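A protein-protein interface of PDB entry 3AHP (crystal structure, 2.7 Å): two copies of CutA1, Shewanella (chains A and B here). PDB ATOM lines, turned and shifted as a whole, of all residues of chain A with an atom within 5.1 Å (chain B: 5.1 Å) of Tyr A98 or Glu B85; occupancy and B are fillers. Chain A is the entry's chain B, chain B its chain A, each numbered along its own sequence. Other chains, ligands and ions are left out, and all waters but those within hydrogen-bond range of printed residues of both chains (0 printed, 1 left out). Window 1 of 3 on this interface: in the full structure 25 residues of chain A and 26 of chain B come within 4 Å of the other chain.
Hydrophobic or aromatic side chains of chain A that line the printed part of chain B: Phe A95 and Tyr A98. Of the 9 printed residues of chain B, 7 touch a printed residue of chain A. Hydrophobic or aromatic side chains of chain B that line the printed part of chain A: Phe B10, Val B83, Pro B84, Phe B86 and Ile B87. Among the printed residues, 11 pairs touch across the chains.
OE2 of Glu B85 is in salt-bridge range of NZ of Lys A62 (2.8 Å). N of Phe A95 is in hydrogen-bond range of O of Phe B86, 3.3 Å away.
Printed residues of chain B within 4 Å of Phe A95: Pro B84 and Phe B86. Of the printed residues of chain B, Pro A97 touches Val B83. Of the printed residues of chain B, Tyr A98 touches Val B83 (3.5 Å), Pro B84 (3.4 Å), Glu B85 (3.6 Å) and Ile B87 (3.9 Å). Of the printed residues of chain A, Phe B10 touches Gln A60. Of the printed residues of chain A, Val B83 touches Pro A97 (3.6 Å) and Tyr A98 (3.5 Å). Glu B85 touches just these residues of chain A: Gln A36, Lys A62 and Tyr A98. Printed residues of chain A within 4 Å of Ile B87: Tyr A98 (3.9 Å). The nearest residue of chain B that does not touch Tyr A98 is Phe B86 (4.04 Å). The nearest residue of chain A that does not touch Glu B85 is Gln A60 (4.2 Å).
Among the printed residues, merely in contact across the chains: Tyr A98 with Pro B84 (3.4 Å), Tyr A98 with Val B83 (3.5 Å), Tyr A98 with Glu B85 (3.6 Å), Pro A97 with Val B83 (3.6 Å), Gln A36 with Thr B12 (3.9 Å), Gln A36 with Glu B85 (3.9 Å), Tyr A98 with Ile B87 (3.9 Å), Gln A60 with Phe B10 (3.9 Å) and Phe A95 with Pro B84 (3.96 Å).
The backbone NH of Phe B10 lies within hydrogen-bond range of the backbone carbonyl oxygen of Ile B87. The backbone carbonyl oxygen (O) of Glu B85 lies within hydrogen-bond range of the side-chain hydroxyl (OG1) of Thr B11, at 2.6 Å. O of Cys A34 sits at hydrogen-bond distance from N of Lys A62 (3.1 Å). O of Gln A36 sits at hydrogen-bond distance from N of Gln A60 (2.9 Å). NE2 of Gln A60 sits close to NZ of Lys A62, at 3.0 Å.
No position is printed for both chains. Of the 11 pairs that touch across the chains among the printed residues, none has its exchanged pair printed and touching as well.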
ATOM      1  N   CYS A  34     -25.656 -18.223  19.322  1.00  0.00           N
ATOM      2  CA  CYS A  34     -25.094 -16.992  19.859  1.00  0.00           C
ATOM      3  C   CYS A  34     -26.062 -16.224  20.744  1.00  0.00           C
ATOM      4  O   CYS A  34     -27.265 -16.111  20.443  1.00  0.00           O
ATOM      5  CB  CYS A  34     -24.617 -16.070  18.746  1.00  0.00           C
ATOM      6  SG  CYS A  34     -24.112 -14.451  19.366  1.00  0.00           S
ATOM      7  N   GLN A  36     -26.314 -12.455  23.078  1.00  0.00           N
ATOM      8  CA  GLN A  36     -25.776 -11.110  23.248  1.00  0.00           C
ATOM      9  C   GLN A  36     -26.294 -10.538  24.553  1.00  0.00           C
ATOM     10  O   GLN A  36     -27.492 -10.548  24.814  1.00  0.00           O
ATOM     11  CB  GLN A  36     -26.216 -10.240  22.065  1.00  0.00           C
ATOM     12  CG  GLN A  36     -25.637  -8.833  22.009  1.00  0.00           C
ATOM     13  CD  GLN A  36     -26.260  -7.996  20.884  1.00  0.00           C
ATOM     14  OE1 GLN A  36     -26.069  -8.282  19.702  1.00  0.00           O
ATOM     15  NE2 GLN A  36     -27.065  -7.003  21.258  1.00  0.00           N
ATOM     16  N   GLN A  60     -30.154 -10.745  23.756  1.00  0.00           N
ATOM     17  CA  GLN A  60     -30.666 -11.250  22.487  1.00  0.00           C
ATOM     18  C   GLN A  60     -30.210 -12.686  22.235  1.00  0.00           C
ATOM     19  O   GLN A  60     -29.026 -12.974  22.283  1.00  0.00           O
ATOM     20  CB  GLN A  60     -30.201 -10.385  21.322  1.00  0.00           C
ATOM     21  CG  GLN A  60     -30.685  -8.939  21.305  1.00  0.00           C
ATOM     22  CD  GLN A  60     -30.147  -8.192  20.078  1.00  0.00           C
ATOM     23  OE1 GLN A  60     -30.368  -6.986  19.926  1.00  0.00           O
ATOM     24  NE2 GLN A  60     -29.414  -8.919  19.202  1.00  0.00           N
ATOM     25  N   LYS A  62     -30.143 -15.807  19.429  1.00  0.00           N
ATOM     26  CA  LYS A  62     -30.401 -16.187  18.060  1.00  0.00           C
ATOM     27  C   LYS A  62     -30.382 -17.688  17.919  1.00  0.00           C
ATOM     28  O   LYS A  62     -29.439 -18.352  18.364  1.00  0.00           O
ATOM     29  CB  LYS A  62     -29.428 -15.503  17.101  1.00  0.00           C
ATOM     30  CG  LYS A  62     -29.572 -13.986  17.092  1.00  0.00           C
ATOM     31  CD  LYS A  62     -28.220 -13.309  17.062  1.00  0.00           C
ATOM     32  CE  LYS A  62     -27.779 -12.843  18.435  1.00  0.00           C
ATOM     33  NZ  LYS A  62     -27.849 -11.347  18.521  1.00  0.00           N
ATOM     34  N   PHE A  95     -27.671 -12.678   6.246  1.00  0.00           N
ATOM     35  CA  PHE A  95     -26.550 -13.285   5.556  1.00  0.00           C
ATOM     36  C   PHE A  95     -26.664 -14.799   5.569  1.00  0.00           C
ATOM     37  O   PHE A  95     -26.496 -15.419   6.609  1.00  0.00           O
ATOM     38  CB  PHE A  95     -25.216 -12.842   6.156  1.00  0.00           C
ATOM     39  CG  PHE A  95     -24.037 -13.149   5.285  1.00  0.00           C
ATOM     40  CD1 PHE A  95     -24.121 -13.002   3.902  1.00  0.00           C
ATOM     41  CD2 PHE A  95     -22.861 -13.638   5.829  1.00  0.00           C
ATOM     42  CE1 PHE A  95     -23.051 -13.331   3.078  1.00  0.00           C
ATOM     43  CE2 PHE A  95     -21.776 -13.946   5.016  1.00  0.00           C
ATOM     44  CZ  PHE A  95     -21.870 -13.777   3.632  1.00  0.00           C
ATOM     45  N   GLY A  96     -26.940 -15.381   4.404  1.00  0.00           N
ATOM     46  CA  GLY A  96     -27.043 -16.833   4.229  1.00  0.00           C
ATOM     47  C   GLY A  96     -26.114 -17.701   5.060  1.00  0.00           C
ATOM     48  O   GLY A  96     -26.578 -18.639   5.707  1.00  0.00           O
ATOM     49  N   PRO A  97     -24.793 -17.430   5.013  1.00  0.00           N
ATOM     50  CA  PRO A  97     -23.826 -18.253   5.749  1.00  0.00           C
ATOM     51  C   PRO A  97     -23.896 -18.093   7.269  1.00  0.00           C
ATOM     52  O   PRO A  97     -23.463 -18.989   8.002  1.00  0.00           O
ATOM     53  CB  PRO A  97     -22.461 -17.766   5.229  1.00  0.00           C
ATOM     54  CG  PRO A  97     -22.743 -17.191   3.907  1.00  0.00           C
ATOM     55  CD  PRO A  97     -24.125 -16.582   4.013  1.00  0.00           C
ATOM     56  N   TYR A  98     -24.386 -16.966   7.749  1.00  0.00           N
ATOM     57  CA  TYR A  98     -24.703 -16.810   9.151  1.00  0.00           C
ATOM     58  C   TYR A  98     -25.896 -17.610   9.576  1.00  0.00           C
ATOM     59  O   TYR A  98     -25.906 -18.177  10.612  1.00  0.00           O
ATOM     60  CB  TYR A  98     -24.896 -15.356   9.533  1.00  0.00           C
ATOM     61  CG  TYR A  98     -25.072 -15.144  11.012  1.00  0.00           C
ATOM     62  CD1 TYR A  98     -26.267 -14.836  11.534  1.00  0.00           C
ATOM     63  CD2 TYR A  98     -24.031 -15.253  11.862  1.00  0.00           C
ATOM     64  CE1 TYR A  98     -26.416 -14.665  12.851  1.00  0.00           C
ATOM     65  CE2 TYR A  98     -24.175 -15.062  13.154  1.00  0.00           C
ATOM     66  CZ  TYR A  98     -25.368 -14.779  13.662  1.00  0.00           C
ATOM     67  OH  TYR A  98     -25.506 -14.584  14.984  1.00  0.00           O
ATOM     68  N   LEU A  99     -26.899 -17.689   8.747  1.00  0.00           N
ATOM     69  CA  LEU A  99     -28.070 -18.385   9.120  1.00  0.00           C
ATOM     70  C   LEU A  99     -27.854 -19.867   9.094  1.00  0.00           C
ATOM     71  O   LEU A  99     -28.323 -20.580   9.941  1.00  0.00           O
ATOM     72  CB  LEU A  99     -29.218 -17.965   8.229  1.00  0.00           C
ATOM     73  CG  LEU A  99     -29.569 -16.493   8.066  1.00  0.00           C
ATOM     74  CD1 LEU A  99     -30.713 -16.334   7.158  1.00  0.00           C
ATOM     75  CD2 LEU A  99     -29.854 -15.816   9.344  1.00  0.00           C
ATOM     76  N   GLN A 100     -27.138 -20.317   8.094  1.00  0.00           N
ATOM     77  CA  GLN A 100     -26.511 -21.606   8.081  1.00  0.00           C
ATOM     78  C   GLN A 100     -25.810 -21.960   9.359  1.00  0.00           C
ATOM     79  O   GLN A 100     -26.064 -22.979   9.914  1.00  0.00           O
ATOM     80  CB  GLN A 100     -25.545 -21.658   6.921  1.00  0.00           C
ATOM     81  CG  GLN A 100     -25.297 -23.008   6.323  1.00  0.00           C
ATOM     82  CD  GLN A 100     -26.527 -23.778   6.036  1.00  0.00           C
ATOM     83  OE1 GLN A 100     -26.840 -24.714   6.723  1.00  0.00           O
ATOM     84  NE2 GLN A 100     -27.216 -23.412   4.993  1.00  0.00           N
ATOM     85  N   TRP A 101     -24.907 -21.117   9.807  1.00  0.00           N
ATOM     86  CA  TRP A 101     -24.121 -21.396  10.999  1.00  0.00           C
ATOM     87  C   TRP A 101     -24.999 -21.664  12.203  1.00  0.00           C
ATOM     88  O   TRP A 101     -24.731 -22.589  12.974  1.00  0.00           O
ATOM     89  CB  TRP A 101     -23.196 -20.229  11.306  1.00  0.00           C
ATOM     90  CG  TRP A 101     -22.472 -20.341  12.617  1.00  0.00           C
ATOM     91  CD1 TRP A 101     -21.514 -21.253  12.946  1.00  0.00           C
ATOM     92  CD2 TRP A 101     -22.573 -19.448  13.733  1.00  0.00           C
ATOM     93  NE1 TRP A 101     -21.022 -20.995  14.206  1.00  0.00           N
ATOM     94  CE2 TRP A 101     -21.658 -19.894  14.711  1.00  0.00           C
ATOM     95  CE3 TRP A 101     -23.342 -18.305  13.996  1.00  0.00           C
ATOM     96  CZ2 TRP A 101     -21.486 -19.237  15.931  1.00  0.00           C
ATOM     97  CZ3 TRP A 101     -23.198 -17.676  15.221  1.00  0.00           C
ATOM     98  CH2 TRP A 101     -22.275 -18.145  16.175  1.00  0.00           C
ATOM     99  N   ILE A 102     -26.018 -20.819  12.369  1.00  0.00           N
ATOM    100  CA  ILE A 102     -27.097 -21.048  13.316  1.00  0.00           C
ATOM    101  C   ILE A 102     -27.736 -22.396  13.110  1.00  0.00           C
ATOM    102  O   ILE A 102     -27.959 -23.121  14.061  1.00  0.00           O
ATOM    103  CB  ILE A 102     -28.191 -19.971  13.203  1.00  0.00           C
ATOM    104  CG1 ILE A 102     -27.603 -18.590  13.513  1.00  0.00           C
ATOM    105  CG2 ILE A 102     -29.351 -20.297  14.141  1.00  0.00           C
ATOM    106  CD1 ILE A 102     -28.592 -17.419  13.347  1.00  0.00           C
ATOM    107  N   PHE B  10     -30.405  -6.281  12.336  1.00  0.00           N
ATOM    108  CA  PHE B  10     -29.469  -6.305  13.450  1.00  0.00           C
ATOM    109  C   PHE B  10     -28.096  -6.807  13.004  1.00  0.00           C
ATOM    110  O   PHE B  10     -27.966  -7.776  12.249  1.00  0.00           O
ATOM    111  CB  PHE B  10     -30.002  -7.162  14.623  1.00  0.00           C
ATOM    112  CG  PHE B  10     -31.274  -6.634  15.242  1.00  0.00           C
ATOM    113  CD1 PHE B  10     -32.518  -6.954  14.698  1.00  0.00           C
ATOM    114  CD2 PHE B  10     -31.226  -5.778  16.335  1.00  0.00           C
ATOM    115  CE1 PHE B  10     -33.683  -6.448  15.245  1.00  0.00           C
ATOM    116  CE2 PHE B  10     -32.389  -5.292  16.912  1.00  0.00           C
ATOM    117  CZ  PHE B  10     -33.617  -5.637  16.372  1.00  0.00           C
ATOM    118  N   THR B  11     -27.059  -6.140  13.474  1.00  0.00           N
ATOM    119  CA  THR B  11     -25.720  -6.559  13.117  1.00  0.00           C
ATOM    120  C   THR B  11     -24.746  -6.109  14.178  1.00  0.00           C
ATOM    121  O   THR B  11     -25.087  -5.340  15.072  1.00  0.00           O
ATOM    122  CB  THR B  11     -25.293  -6.035  11.699  1.00  0.00           C
ATOM    123  OG1 THR B  11     -24.080  -6.676  11.287  1.00  0.00           O
ATOM    124  CG2 THR B  11     -25.104  -4.527  11.688  1.00  0.00           C
ATOM    125  N   THR B  12     -23.520  -6.585  14.050  1.00  0.00           N
ATOM    126  CA  THR B  12     -22.521  -6.414  15.076  1.00  0.00           C
ATOM    127  C   THR B  12     -21.193  -6.088  14.406  1.00  0.00           C
ATOM    128  O   THR B  12     -20.866  -6.666  13.391  1.00  0.00           O
ATOM    129  CB  THR B  12     -22.458  -7.700  15.921  1.00  0.00           C
ATOM    130  OG1 THR B  12     -23.416  -7.611  16.988  1.00  0.00           O
ATOM    131  CG2 THR B  12     -21.101  -7.925  16.476  1.00  0.00           C
ATOM    132  N   SER B  43     -21.017 -10.681  23.192  1.00  0.00           N
ATOM    133  CA  SER B  43     -21.522 -11.804  22.419  1.00  0.00           C
ATOM    134  C   SER B  43     -20.911 -13.106  22.913  1.00  0.00           C
ATOM    135  O   SER B  43     -19.708 -13.196  23.110  1.00  0.00           O
ATOM    136  CB  SER B  43     -21.235 -11.608  20.927  1.00  0.00           C
ATOM    137  OG  SER B  43     -21.947 -10.486  20.417  1.00  0.00           O
ATOM    138  N   VAL B  83     -17.943 -14.387   8.220  1.00  0.00           N
ATOM    139  CA  VAL B  83     -19.396 -14.533   8.350  1.00  0.00           C
ATOM    140  C   VAL B  83     -19.973 -13.863   9.587  1.00  0.00           C
ATOM    141  O   VAL B  83     -20.115 -14.478  10.628  1.00  0.00           O
ATOM    142  CB  VAL B  83     -19.912 -15.997   8.118  1.00  0.00           C
ATOM    143  CG1 VAL B  83     -18.822 -17.034   8.374  1.00  0.00           C
ATOM    144  CG2 VAL B  83     -21.188 -16.283   8.903  1.00  0.00           C
ATOM    145  N   PRO B  84     -20.255 -12.561   9.474  1.00  0.00           N
ATOM    146  CA  PRO B  84     -20.644 -11.734  10.606  1.00  0.00           C
ATOM    147  C   PRO B  84     -22.130 -11.902  10.900  1.00  0.00           C
ATOM    148  O   PRO B  84     -22.849 -12.529  10.122  1.00  0.00           O
ATOM    149  CB  PRO B  84     -20.355 -10.301  10.113  1.00  0.00           C
ATOM    150  CG  PRO B  84     -19.925 -10.417   8.654  1.00  0.00           C
ATOM    151  CD  PRO B  84     -20.286 -11.801   8.211  1.00  0.00           C
ATOM    152  N   GLU B  85     -22.569 -11.401  12.046  1.00  0.00           N
ATOM    153  CA  GLU B  85     -23.974 -11.483  12.394  1.00  0.00           C
ATOM    154  C   GLU B  85     -24.746 -10.425  11.615  1.00  0.00           C
ATOM    155  O   GLU B  85     -24.346  -9.261  11.533  1.00  0.00           O
ATOM    156  CB  GLU B  85     -24.171 -11.341  13.905  1.00  0.00           C
ATOM    157  CG  GLU B  85     -25.584 -11.023  14.376  1.00  0.00           C
ATOM    158  CD  GLU B  85     -25.656 -10.780  15.893  1.00  0.00           C
ATOM    159  OE1 GLU B  85     -24.766 -11.272  16.629  1.00  0.00           O
ATOM    160  OE2 GLU B  85     -26.617 -10.123  16.351  1.00  0.00           O
ATOM    161  N   PHE B  86     -25.790 -10.872  10.939  1.00  0.00           N
ATOM    162  CA  PHE B  86     -26.554 -10.002  10.084  1.00  0.00           C
ATOM    163  C   PHE B  86     -27.919 -10.635   9.902  1.00  0.00           C
ATOM    164  O   PHE B  86     -28.023 -11.719   9.341  1.00  0.00           O
ATOM    165  CB  PHE B  86     -25.833  -9.836   8.744  1.00  0.00           C
ATOM    166  CG  PHE B  86     -26.365  -8.726   7.900  1.00  0.00           C
ATOM    167  CD1 PHE B  86     -25.958  -7.404   8.120  1.00  0.00           C
ATOM    168  CD2 PHE B  86     -27.265  -8.993   6.879  1.00  0.00           C
ATOM    169  CE1 PHE B  86     -26.417  -6.363   7.301  1.00  0.00           C
ATOM    170  CE2 PHE B  86     -27.752  -7.962   6.072  1.00  0.00           C
ATOM    171  CZ  PHE B  86     -27.297  -6.645   6.260  1.00  0.00           C
ATOM    172  N   ILE B  87     -28.938 -10.057  10.525  1.00  0.00           N
ATOM    173  CA  ILE B  87     -30.259 -10.670  10.486  1.00  0.00           C
ATOM    174  C   ILE B  87     -31.367  -9.657  10.218  1.00  0.00           C
ATOM    175  O   ILE B  87     -31.290  -8.505  10.632  1.00  0.00           O
ATOM    176  CB  ILE B  87     -30.565 -11.504  11.752  1.00  0.00           C
ATOM    177  CG1 ILE B  87     -30.513 -10.627  12.993  1.00  0.00           C
ATOM    178  CG2 ILE B  87     -29.579 -12.657  11.890  1.00  0.00           C
ATOM    179  CD1 ILE B  87     -31.199 -11.239  14.186  1.00  0.00           C
